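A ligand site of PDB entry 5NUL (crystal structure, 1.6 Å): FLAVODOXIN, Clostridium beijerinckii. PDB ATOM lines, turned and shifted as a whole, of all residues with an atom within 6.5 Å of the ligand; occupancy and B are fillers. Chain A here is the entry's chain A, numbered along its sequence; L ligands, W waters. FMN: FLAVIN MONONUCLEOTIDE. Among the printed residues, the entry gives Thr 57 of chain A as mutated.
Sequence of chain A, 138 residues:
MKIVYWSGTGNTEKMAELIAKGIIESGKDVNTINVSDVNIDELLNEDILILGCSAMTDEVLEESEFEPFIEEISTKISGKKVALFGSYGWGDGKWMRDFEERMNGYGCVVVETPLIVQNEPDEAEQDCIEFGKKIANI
The backbone carbonyl oxygen (O) of Ser 54 is in hydrogen-bond range of the indole nitrogen (NE1) of Trp 95, at 3.4 Å. The side-chain amide nitrogen (ND2) of Asn 119 sits close to the side-chain amide nitrogen (NE2) of Gln 118, 3.5 Å away. OG1 of Thr 9 sits at hydrogen-bond distance from OD1 of Asn 11, at 3.5 Å. OG of Ser 7 sits at hydrogen-bond distance from N of Thr 12. The backbone NH of Asn 119 sits at hydrogen-bond distance from the backbone carbonyl oxygen of Tyr 88 (2.8 Å). OE1 of Glu 59 is in hydrogen-bond range of N of Trp 95 (2.9 Å). The side-chain hydroxyl of Thr 12 sits close to the backbone NH of Ser 54, at 3.5 Å. The side-chain hydroxyl (OG) of Ser 7 is in hydrogen-bond range of the backbone NH (N) of Asn 11.
The backbone carbonyl oxygen (O) of Thr 57 sits close to a nitrogen (N5) of the ligand, 2.8 Å away. Merely in contact with the ligand: Trp 6, Met 56, Asp 58, Tyr 88 and Asn 119. Hydrophobic or aromatic side chains that line the ligand: Trp 6, Ala 55, Met 56, Tyr 88 and Trp 90. 19 residues have an atom within 4 Å of the ligand: Trp 6, Ser 7, Gly 8, Thr 9, Gly 10, Asn 11, Thr 12, Ser 54, Ala 55, Met 56, Thr 57, Asp 58, Glu 59, Ser 87, Tyr 88, Gly 89, Trp 90, Gly 91 and Asn 119.
OG of Ser 7 lies within hydrogen-bond range of O2P of the ligand (2.7 Å). The backbone NH (N) of Ala 55 lies within hydrogen-bond range of an oxygen (O2') of the ligand (3.4 Å). OD1 of Asn 11 lies within hydrogen-bond range of O4' of the ligand, 2.9 Å away. N of Gly 89 lies within hydrogen-bond range of O2 of the ligand, at 3.0 Å. The backbone NH (N) of Glu 59 sits at hydrogen-bond distance from an oxygen (O4) of the ligand. O4' of the ligand is in hydrogen-bond range of OG of Ser 87 (2.7 Å). OG of Ser 54 lies within hydrogen-bond range of O1P of the ligand, 2.8 Å away. An oxygen (O2P) of the ligand lies within hydrogen-bond range of the backbone NH of Thr 12. A nitrogen (N3) of the ligand is in hydrogen-bond range of the side-chain carboxylate of Glu 59 (2.9 Å). The side-chain hydroxyl (OG1) of Thr 9 sits at hydrogen-bond distance from an oxygen (O3P) of the ligand (2.7 Å). The backbone NH of Gly 91 is in hydrogen-bond range of an oxygen (O2) of the ligand, 2.8 Å away. An oxygen (O3P) of the ligand is in hydrogen-bond range of the backbone NH of Thr 9, 2.8 Å away. The backbone NH of Trp 90 is in hydrogen-bond range of an oxygen (O2) of the ligand (3.3 Å). The backbone NH (N) of Gly 10 is in hydrogen-bond range of an oxygen (O3P) of the ligand (3.0 Å). O3P of the ligand sits at hydrogen-bond distance from N of Asn 11 (2.9 Å). O of Ala 55 is in hydrogen-bond range of O2' of the ligand, 2.8 Å away. An oxygen (O1P) of the ligand is in hydrogen-bond range of the backbone NH of Gly 8, at 2.8 Å. O2P of the ligand is in hydrogen-bond range of OG1 of Thr 12 (2.8 Å).
Water W4 lies within hydrogen-bond range of an oxygen (O3') of the ligand and the side-chain amide oxygen of Asn 119. Water W5 lies within hydrogen-bond range of an oxygen (O4) of the ligand, the side-chain carboxylate of Asp 58 and the indole nitrogen of Trp 90. Water W1 lies within hydrogen-bond range of OE1 of Glu 59 (2.8 Å), N of Gly 93 (2.9 Å), O2 of the ligand (3.2 Å) and N of Asp 92 (3.4 Å).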
ATOM      1  N   TRP A   6      29.467  -1.209 -11.929  1.00  0.00           N
ATOM      2  CA  TRP A   6      29.050  -0.403 -13.081  1.00  0.00           C
ATOM      3  C   TRP A   6      27.725  -1.044 -13.513  1.00  0.00           C
ATOM      4  O   TRP A   6      27.635  -2.275 -13.582  1.00  0.00           O
ATOM      5  CB  TRP A   6      30.031  -0.458 -14.263  1.00  0.00           C
ATOM      6  CG  TRP A   6      29.586   0.475 -15.382  1.00  0.00           C
ATOM      7  CD1 TRP A   6      29.859   1.807 -15.486  1.00  0.00           C
ATOM      8  CD2 TRP A   6      28.702   0.167 -16.474  1.00  0.00           C
ATOM      9  NE1 TRP A   6      29.193   2.355 -16.561  1.00  0.00           N
ATOM     10  CE2 TRP A   6      28.474   1.375 -17.185  1.00  0.00           C
ATOM     11  CE3 TRP A   6      28.071  -1.011 -16.920  1.00  0.00           C
ATOM     12  CZ2 TRP A   6      27.643   1.436 -18.311  1.00  0.00           C
ATOM     13  CZ3 TRP A   6      27.233  -0.941 -18.047  1.00  0.00           C
ATOM     14  CH2 TRP A   6      27.033   0.274 -18.727  1.00  0.00           C
ATOM     15  N   SER A   7      26.718  -0.227 -13.798  1.00  0.00           N
ATOM     16  CA  SER A   7      25.422  -0.705 -14.257  1.00  0.00           C
ATOM     17  C   SER A   7      24.864   0.265 -15.314  1.00  0.00           C
ATOM     18  O   SER A   7      24.840   1.475 -15.082  1.00  0.00           O
ATOM     19  CB  SER A   7      24.465  -0.826 -13.066  1.00  0.00           C
ATOM     20  OG  SER A   7      23.240  -1.457 -13.428  1.00  0.00           O
ATOM     21  N   GLY A   8      24.441  -0.269 -16.459  1.00  0.00           N
ATOM     22  CA  GLY A   8      23.897   0.578 -17.514  1.00  0.00           C
ATOM     23  C   GLY A   8      22.400   0.810 -17.453  1.00  0.00           C
ATOM     24  O   GLY A   8      21.914   1.833 -17.931  1.00  0.00           O
ATOM     25  N   THR A   9      21.650  -0.144 -16.909  1.00  0.00           N
ATOM     26  CA  THR A   9      20.200   0.000 -16.808  1.00  0.00           C
ATOM     27  C   THR A   9      19.675  -0.241 -15.382  1.00  0.00           C
ATOM     28  O   THR A   9      18.469  -0.118 -15.123  1.00  0.00           O
ATOM     29  CB  THR A   9      19.426  -0.940 -17.804  1.00  0.00           C
ATOM     30  OG1 THR A   9      19.410  -2.297 -17.307  1.00  0.00           O
ATOM     31  CG2 THR A   9      20.081  -0.910 -19.185  1.00  0.00           C
ATOM     32  N   GLY A  10      20.578  -0.591 -14.476  1.00  0.00           N
ATOM     33  CA  GLY A  10      20.202  -0.820 -13.096  1.00  0.00           C
ATOM     34  C   GLY A  10      20.221  -2.265 -12.647  1.00  0.00           C
ATOM     35  O   GLY A  10      20.071  -2.521 -11.458  1.00  0.00           O
ATOM     36  N   ASN A  11      20.471  -3.214 -13.545  1.00  0.00           N
ATOM     37  CA  ASN A  11      20.441  -4.621 -13.135  1.00  0.00           C
ATOM     38  C   ASN A  11      21.577  -5.018 -12.185  1.00  0.00           C
ATOM     39  O   ASN A  11      21.334  -5.619 -11.120  1.00  0.00           O
ATOM     40  CB  ASN A  11      20.365  -5.551 -14.346  1.00  0.00           C
ATOM     41  CG  ASN A  11      19.099  -5.354 -15.148  1.00  0.00           C
ATOM     42  OD1 ASN A  11      19.062  -5.632 -16.346  1.00  0.00           O
ATOM     43  ND2 ASN A  11      18.054  -4.862 -14.491  1.00  0.00           N
ATOM     44  N   THR A  12      22.798  -4.655 -12.552  1.00  0.00           N
ATOM     45  CA  THR A  12      23.956  -4.911 -11.707  1.00  0.00           C
ATOM     46  C   THR A  12      23.882  -4.041 -10.435  1.00  0.00           C
ATOM     47  O   THR A  12      24.333  -4.457  -9.382  1.00  0.00           O
ATOM     48  CB  THR A  12      25.263  -4.667 -12.465  1.00  0.00           C
ATOM     49  OG1 THR A  12      25.271  -5.538 -13.607  1.00  0.00           O
ATOM     50  CG2 THR A  12      26.469  -5.033 -11.595  1.00  0.00           C
ATOM     51  N   GLU A  13      23.290  -2.842 -10.553  1.00  0.00           N
ATOM     52  CA  GLU A  13      23.118  -1.971  -9.386  1.00  0.00           C
ATOM     53  C   GLU A  13      22.204  -2.661  -8.366  1.00  0.00           C
ATOM     54  O   GLU A  13      22.494  -2.659  -7.163  1.00  0.00           O
ATOM     55  CB  GLU A  13      22.516  -0.625  -9.817  1.00  0.00           C
ATOM     56  CG  GLU A  13      22.383   0.355  -8.656  1.00  0.00           C
ATOM     57  CD  GLU A  13      21.701   1.674  -9.029  1.00  0.00           C
ATOM     58  OE1 GLU A  13      21.178   1.809 -10.149  1.00  0.00           O
ATOM     59  OE2 GLU A  13      21.684   2.573  -8.164  1.00  0.00           O
ATOM     60  N   CYS A  53      30.036  -5.838 -12.705  1.00  0.00           N
ATOM     61  CA  CYS A  53      29.845  -5.177 -13.998  1.00  0.00           C
ATOM     62  C   CYS A  53      29.090  -6.113 -14.928  1.00  0.00           C
ATOM     63  O   CYS A  53      29.375  -7.309 -14.980  1.00  0.00           O
ATOM     64  CB  CYS A  53      31.187  -4.831 -14.633  1.00  0.00           C
ATOM     65  SG  CYS A  53      31.020  -3.891 -16.174  1.00  0.00           S
ATOM     66  N   SER A  54      28.103  -5.568 -15.621  1.00  0.00           N
ATOM     67  CA  SER A  54      27.328  -6.373 -16.554  1.00  0.00           C
ATOM     68  C   SER A  54      28.139  -6.726 -17.816  1.00  0.00           C
ATOM     69  O   SER A  54      29.212  -6.155 -18.066  1.00  0.00           O
ATOM     70  CB  SER A  54      26.073  -5.606 -16.955  1.00  0.00           C
ATOM     71  OG  SER A  54      26.407  -4.298 -17.373  1.00  0.00           O
ATOM     72  N   ALA A  55      27.606  -7.651 -18.604  1.00  0.00           N
ATOM     73  CA  ALA A  55      28.252  -8.065 -19.848  1.00  0.00           C
ATOM     74  C   ALA A  55      28.043  -6.933 -20.868  1.00  0.00           C
ATOM     75  O   ALA A  55      26.917  -6.480 -21.074  1.00  0.00           O
ATOM     76  CB  ALA A  55      27.628  -9.350 -20.364  1.00  0.00           C
ATOM     77  N   MET A  56      29.131  -6.466 -21.465  1.00  0.00           N
ATOM     78  CA  MET A  56      29.063  -5.382 -22.454  1.00  0.00           C
ATOM     79  C   MET A  56      29.615  -5.758 -23.825  1.00  0.00           C
ATOM     80  O   MET A  56      30.329  -6.758 -23.984  1.00  0.00           O
ATOM     81  CB  MET A  56      29.768  -4.129 -21.940  1.00  0.00           C
ATOM     82  CG  MET A  56      28.890  -3.203 -21.097  1.00  0.00           C
ATOM     83  SD  MET A  56      27.531  -2.461 -22.043  1.00  0.00           S
ATOM     84  CE  MET A  56      28.420  -1.821 -23.476  1.00  0.00           C
ATOM     85  N   THR A  57      29.280  -4.925 -24.809  1.00  0.00           N
ATOM     86  CA  THR A  57      29.681  -5.089 -26.199  1.00  0.00           C
ATOM     87  C   THR A  57      29.550  -6.577 -26.546  1.00  0.00           C
ATOM     88  O   THR A  57      28.442  -7.112 -26.545  1.00  0.00           O
ATOM     89  CB  THR A  57      31.117  -4.551 -26.425  1.00  0.00           C
ATOM     90  OG1 THR A  57      31.260  -3.290 -25.750  1.00  0.00           O
ATOM     91  CG2 THR A  57      31.367  -4.340 -27.919  1.00  0.00           C
ATOM     92  N   ASP A  58      30.668  -7.253 -26.821  1.00  0.00           N
ATOM     93  CA  ASP A  58      30.603  -8.682 -27.086  1.00  0.00           C
ATOM     94  C   ASP A  58      31.355  -9.436 -25.989  1.00  0.00           C
ATOM     95  O   ASP A  58      32.553  -9.713 -26.105  1.00  0.00           O
ATOM     96  CB  ASP A  58      31.172  -9.022 -28.463  1.00  0.00           C
ATOM     97  CG  ASP A  58      30.974 -10.484 -28.829  1.00  0.00           C
ATOM     98  OD1 ASP A  58      29.989 -11.093 -28.366  1.00  0.00           O
ATOM     99  OD2 ASP A  58      31.814 -11.032 -29.577  1.00  0.00           O
ATOM    100  N   GLU A  59      30.633  -9.694 -24.909  1.00  0.00           N
ATOM    101  CA  GLU A  59      31.157 -10.430 -23.764  1.00  0.00           C
ATOM    102  C   GLU A  59      32.427  -9.839 -23.144  1.00  0.00           C
ATOM    103  O   GLU A  59      33.387 -10.570 -22.898  1.00  0.00           O
ATOM    104  CB  GLU A  59      31.415 -11.900 -24.134  1.00  0.00           C
ATOM    105  CG  GLU A  59      30.171 -12.690 -24.531  1.00  0.00           C
ATOM    106  CD  GLU A  59      29.213 -12.958 -23.382  1.00  0.00           C
ATOM    107  OE1 GLU A  59      29.617 -12.869 -22.200  1.00  0.00           O
ATOM    108  OE2 GLU A  59      28.044 -13.272 -23.671  1.00  0.00           O
ATOM    109  N   VAL A  60      32.426  -8.539 -22.883  1.00  0.00           N
ATOM    110  CA  VAL A  60      33.575  -7.897 -22.257  1.00  0.00           C
ATOM    111  C   VAL A  60      33.100  -7.002 -21.125  1.00  0.00           C
ATOM    112  O   VAL A  60      31.891  -6.789 -20.966  1.00  0.00           O
ATOM    113  CB  VAL A  60      34.406  -7.045 -23.263  1.00  0.00           C
ATOM    114  CG1 VAL A  60      34.993  -7.935 -24.330  1.00  0.00           C
ATOM    115  CG2 VAL A  60      33.566  -5.927 -23.857  1.00  0.00           C
ATOM    116  N   GLY A  86      27.821  -9.778 -11.666  1.00  0.00           N
ATOM    117  CA  GLY A  86      27.318  -8.953 -12.740  1.00  0.00           C
ATOM    118  C   GLY A  86      26.089  -9.564 -13.378  1.00  0.00           C
ATOM    119  O   GLY A  86      25.835 -10.762 -13.239  1.00  0.00           O
ATOM    120  N   SER A  87      25.317  -8.730 -14.059  1.00  0.00           N
ATOM    121  CA  SER A  87      24.119  -9.180 -14.753  1.00  0.00           C
ATOM    122  C   SER A  87      24.474  -9.343 -16.230  1.00  0.00           C
ATOM    123  O   SER A  87      25.404  -8.700 -16.725  1.00  0.00           O
ATOM    124  CB  SER A  87      23.005  -8.145 -14.578  1.00  0.00           C
ATOM    125  OG  SER A  87      21.812  -8.554 -15.244  1.00  0.00           O
ATOM    126  N   TYR A  88      23.746 -10.213 -16.933  1.00  0.00           N
ATOM    127  CA  TYR A  88      23.992 -10.459 -18.353  1.00  0.00           C
ATOM    128  C   TYR A  88      22.664 -10.741 -19.043  1.00  0.00           C
ATOM    129  O   TYR A  88      21.633 -10.891 -18.388  1.00  0.00           O
ATOM    130  CB  TYR A  88      24.971 -11.621 -18.564  1.00  0.00           C
ATOM    131  CG  TYR A  88      24.432 -12.956 -18.117  1.00  0.00           C
ATOM    132  CD1 TYR A  88      24.344 -13.283 -16.760  1.00  0.00           C
ATOM    133  CD2 TYR A  88      23.996 -13.909 -19.055  1.00  0.00           C
ATOM    134  CE1 TYR A  88      23.845 -14.509 -16.347  1.00  0.00           C
ATOM    135  CE2 TYR A  88      23.497 -15.135 -18.655  1.00  0.00           C
ATOM    136  CZ  TYR A  88      23.433 -15.434 -17.290  1.00  0.00           C
ATOM    137  OH  TYR A  88      22.952 -16.649 -16.896  1.00  0.00           O
ATOM    138  N   GLY A  89      22.699 -10.810 -20.365  1.00  0.00           N
ATOM    139  CA  GLY A  89      21.494 -11.039 -21.132  1.00  0.00           C
ATOM    140  C   GLY A  89      21.479 -12.373 -21.848  1.00  0.00           C
ATOM    141  O   GLY A  89      21.301 -13.423 -21.236  1.00  0.00           O
ATOM    142  N   TRP A  90      21.786 -12.329 -23.131  1.00  0.00           N
ATOM    143  CA  TRP A  90      21.750 -13.504 -23.998  1.00  0.00           C
ATOM    144  C   TRP A  90      22.864 -14.550 -23.924  1.00  0.00           C
ATOM    145  O   TRP A  90      22.715 -15.639 -24.445  1.00  0.00           O
ATOM    146  CB  TRP A  90      21.610 -13.046 -25.449  1.00  0.00           C
ATOM    147  CG  TRP A  90      22.688 -12.108 -25.872  1.00  0.00           C
ATOM    148  CD1 TRP A  90      23.915 -12.445 -26.354  1.00  0.00           C
ATOM    149  CD2 TRP A  90      22.653 -10.673 -25.833  1.00  0.00           C
ATOM    150  NE1 TRP A  90      24.640 -11.313 -26.625  1.00  0.00           N
ATOM    151  CE2 TRP A  90      23.890 -10.210 -26.320  1.00  0.00           C
ATOM    152  CE3 TRP A  90      21.690  -9.732 -25.436  1.00  0.00           C
ATOM    153  CZ2 TRP A  90      24.198  -8.854 -26.422  1.00  0.00           C
ATOM    154  CZ3 TRP A  90      21.998  -8.376 -25.537  1.00  0.00           C
ATOM    155  CH2 TRP A  90      23.245  -7.954 -26.023  1.00  0.00           C
ATOM    156  N   GLY A  91      23.996 -14.197 -23.319  1.00  0.00           N
ATOM    157  CA  GLY A  91      25.125 -15.113 -23.245  1.00  0.00           C
ATOM    158  C   GLY A  91      24.983 -16.113 -22.121  1.00  0.00           C
ATOM    159  O   GLY A  91      23.895 -16.319 -21.598  1.00  0.00           O
ATOM    160  N   ASP A  92      26.089 -16.753 -21.760  1.00  0.00           N
ATOM    161  CA  ASP A  92      26.078 -17.715 -20.670  1.00  0.00           C
ATOM    162  C   ASP A  92      27.216 -17.496 -19.689  1.00  0.00           C
ATOM    163  O   ASP A  92      27.692 -18.445 -19.041  1.00  0.00           O
ATOM    164  CB  ASP A  92      26.093 -19.152 -21.192  1.00  0.00           C
ATOM    165  CG  ASP A  92      27.327 -19.478 -22.036  1.00  0.00           C
ATOM    166  OD1 ASP A  92      28.320 -18.707 -22.038  1.00  0.00           O
ATOM    167  OD2 ASP A  92      27.288 -20.525 -22.712  1.00  0.00           O
ATOM    168  N   GLY A  93      27.725 -16.263 -19.641  1.00  0.00           N
ATOM    169  CA  GLY A  93      28.781 -15.944 -18.693  1.00  0.00           C
ATOM    170  C   GLY A  93      30.207 -15.824 -19.201  1.00  0.00           C
ATOM    171  O   GLY A  93      31.122 -15.726 -18.382  1.00  0.00           O
ATOM    172  N   TRP A  95      31.891 -13.329 -20.387  1.00  0.00           N
ATOM    173  CA  TRP A  95      32.560 -12.136 -19.882  1.00  0.00           C
ATOM    174  C   TRP A  95      33.042 -12.342 -18.438  1.00  0.00           C
ATOM    175  O   TRP A  95      34.111 -11.862 -18.058  1.00  0.00           O
ATOM    176  CB  TRP A  95      31.668 -10.896 -20.006  1.00  0.00           C
ATOM    177  CG  TRP A  95      31.023 -10.420 -18.741  1.00  0.00           C
ATOM    178  CD1 TRP A  95      31.334  -9.286 -18.025  1.00  0.00           C
ATOM    179  CD2 TRP A  95      29.919 -11.037 -18.053  1.00  0.00           C
ATOM    180  NE1 TRP A  95      30.484  -9.160 -16.949  1.00  0.00           N
ATOM    181  CE2 TRP A  95      29.610 -10.212 -16.937  1.00  0.00           C
ATOM    182  CE3 TRP A  95      29.162 -12.203 -18.266  1.00  0.00           C
ATOM    183  CZ2 TRP A  95      28.576 -10.520 -16.048  1.00  0.00           C
ATOM    184  CZ3 TRP A  95      28.128 -12.499 -17.384  1.00  0.00           C
ATOM    185  CH2 TRP A  95      27.839 -11.661 -16.288  1.00  0.00           C
ATOM    186  N   VAL A 117      23.711 -13.135 -12.877  1.00  0.00           N
ATOM    187  CA  VAL A 117      22.248 -13.186 -12.918  1.00  0.00           C
ATOM    188  C   VAL A 117      21.743 -12.615 -14.231  1.00  0.00           C
ATOM    189  O   VAL A 117      22.252 -11.589 -14.692  1.00  0.00           O
ATOM    190  CB  VAL A 117      21.634 -12.393 -11.738  1.00  0.00           C
ATOM    191  CG1 VAL A 117      20.140 -12.220 -11.917  1.00  0.00           C
ATOM    192  CG2 VAL A 117      21.926 -13.118 -10.417  1.00  0.00           C
ATOM    193  N   GLN A 118      20.777 -13.291 -14.837  1.00  0.00           N
ATOM    194  CA  GLN A 118      20.214 -12.841 -16.111  1.00  0.00           C
ATOM    195  C   GLN A 118      19.212 -11.707 -15.923  1.00  0.00           C
ATOM    196  O   GLN A 118      18.233 -11.854 -15.186  1.00  0.00           O
ATOM    197  CB  GLN A 118      19.562 -14.012 -16.856  1.00  0.00           C
ATOM    198  CG  GLN A 118      19.379 -13.752 -18.344  1.00  0.00           C
ATOM    199  CD  GLN A 118      18.723 -14.902 -19.096  1.00  0.00           C
ATOM    200  OE1 GLN A 118      18.834 -16.071 -18.699  1.00  0.00           O
ATOM    201  NE2 GLN A 118      18.052 -14.587 -20.192  1.00  0.00           N
ATOM    202  N   ASN A 119      19.488 -10.582 -16.577  1.00  0.00           N
ATOM    203  CA  ASN A 119      18.624  -9.399 -16.529  1.00  0.00           C
ATOM    204  C   ASN A 119      18.395  -8.925 -15.095  1.00  0.00           C
ATOM    205  O   ASN A 119      19.285  -9.047 -14.262  1.00  0.00           O
ATOM    206  CB  ASN A 119      17.299  -9.670 -17.254  1.00  0.00           C
ATOM    207  CG  ASN A 119      17.511 -10.343 -18.610  1.00  0.00           C
ATOM    208  OD1 ASN A 119      18.097  -9.770 -19.532  1.00  0.00           O
ATOM    209  ND2 ASN A 119      17.064 -11.586 -18.725  1.00  0.00           N
ATOM    210  N   GLU A 120      17.225  -8.366 -14.787  1.00  0.00           N
ATOM    211  CA  GLU A 120      17.006  -7.914 -13.415  1.00  0.00           C
ATOM    212  C   GLU A 120      16.915  -9.145 -12.528  1.00  0.00           C
ATOM    213  O   GLU A 120      16.307 -10.147 -12.909  1.00  0.00           O
ATOM    214  CB  GLU A 120      15.735  -7.047 -13.293  1.00  0.00           C
ATOM    215  CG  GLU A 120      15.837  -6.076 -12.108  1.00  0.00           C
ATOM    216  CD  GLU A 120      14.525  -5.415 -11.711  1.00  0.00           C
ATOM    217  OE1 GLU A 120      13.912  -4.737 -12.572  1.00  0.00           O
ATOM    218  OE2 GLU A 120      14.119  -5.554 -10.533  1.00  0.00           O
HETATM  219  N1  FMN L   1      24.680  -9.698 -22.373  1.00  0.00           N
HETATM  220  C2  FMN L   1      25.318 -10.872 -22.585  1.00  0.00           C
HETATM  221  O2  FMN L   1      24.923 -11.905 -22.095  1.00  0.00           O
HETATM  222  N3  FMN L   1      26.454 -10.876 -23.381  1.00  0.00           N
HETATM  223  C4  FMN L   1      26.940  -9.794 -24.085  1.00  0.00           C
HETATM  224  O4  FMN L   1      27.907  -9.884 -24.821  1.00  0.00           O
HETATM  225  C4A FMN L   1      26.208  -8.528 -23.894  1.00  0.00           C
HETATM  226  N5  FMN L   1      26.585  -7.430 -24.527  1.00  0.00           N
HETATM  227  C5A FMN L   1      25.813  -6.278 -24.395  1.00  0.00           C
HETATM  228  C6  FMN L   1      26.114  -5.105 -25.147  1.00  0.00           C
HETATM  229  C7  FMN L   1      25.419  -3.934 -24.946  1.00  0.00           C
HETATM  230  C7M FMN L   1      25.767  -2.680 -25.682  1.00  0.00           C
HETATM  231  C8  FMN L   1      24.331  -3.889 -23.991  1.00  0.00           C
HETATM  232  C8M FMN L   1      23.586  -2.602 -23.681  1.00  0.00           C
HETATM  233  C9  FMN L   1      23.973  -5.045 -23.328  1.00  0.00           C
HETATM  234  C9A FMN L   1      24.699  -6.228 -23.478  1.00  0.00           C
HETATM  235  N10 FMN L   1      24.354  -7.425 -22.841  1.00  0.00           N
HETATM  236  C10 FMN L   1      25.062  -8.596 -22.985  1.00  0.00           C
HETATM  237  C1' FMN L   1      23.150  -7.451 -21.993  1.00  0.00           C
HETATM  238  C2' FMN L   1      23.423  -6.909 -20.582  1.00  0.00           C
HETATM  239  O2' FMN L   1      24.553  -7.544 -19.985  1.00  0.00           O
HETATM  240  C3' FMN L   1      22.177  -7.154 -19.707  1.00  0.00           C
HETATM  241  O3' FMN L   1      21.068  -6.417 -20.240  1.00  0.00           O
HETATM  242  C4' FMN L   1      22.364  -6.809 -18.223  1.00  0.00           C
HETATM  243  O4' FMN L   1      21.167  -7.163 -17.514  1.00  0.00           O
HETATM  244  C5' FMN L   1      22.624  -5.304 -18.059  1.00  0.00           C
HETATM  245  O5' FMN L   1      22.939  -5.025 -16.700  1.00  0.00           O
HETATM  246  P   FMN L   1      23.098  -3.524 -16.245  1.00  0.00           P
HETATM  247  O1P FMN L   1      23.997  -2.890 -17.238  1.00  0.00           O
HETATM  248  O2P FMN L   1      23.635  -3.638 -14.890  1.00  0.00           O
HETATM  249  O3P FMN L   1      21.773  -2.791 -16.147  1.00  0.00           O
HETATM  250  O   HOH W   1      27.269 -13.668 -20.821  1.00  0.00           O
HETATM  251  O   HOH W   2      21.642  -3.768 -20.863  1.00  0.00           O
HETATM  252  O   HOH W   3      23.549  -2.077 -19.732  1.00  0.00           O
HETATM  253  O   HOH W   4      18.527  -7.029 -19.520  1.00  0.00           O
HETATM  254  O   HOH W   5      27.327 -10.705 -27.448  1.00  0.00           O
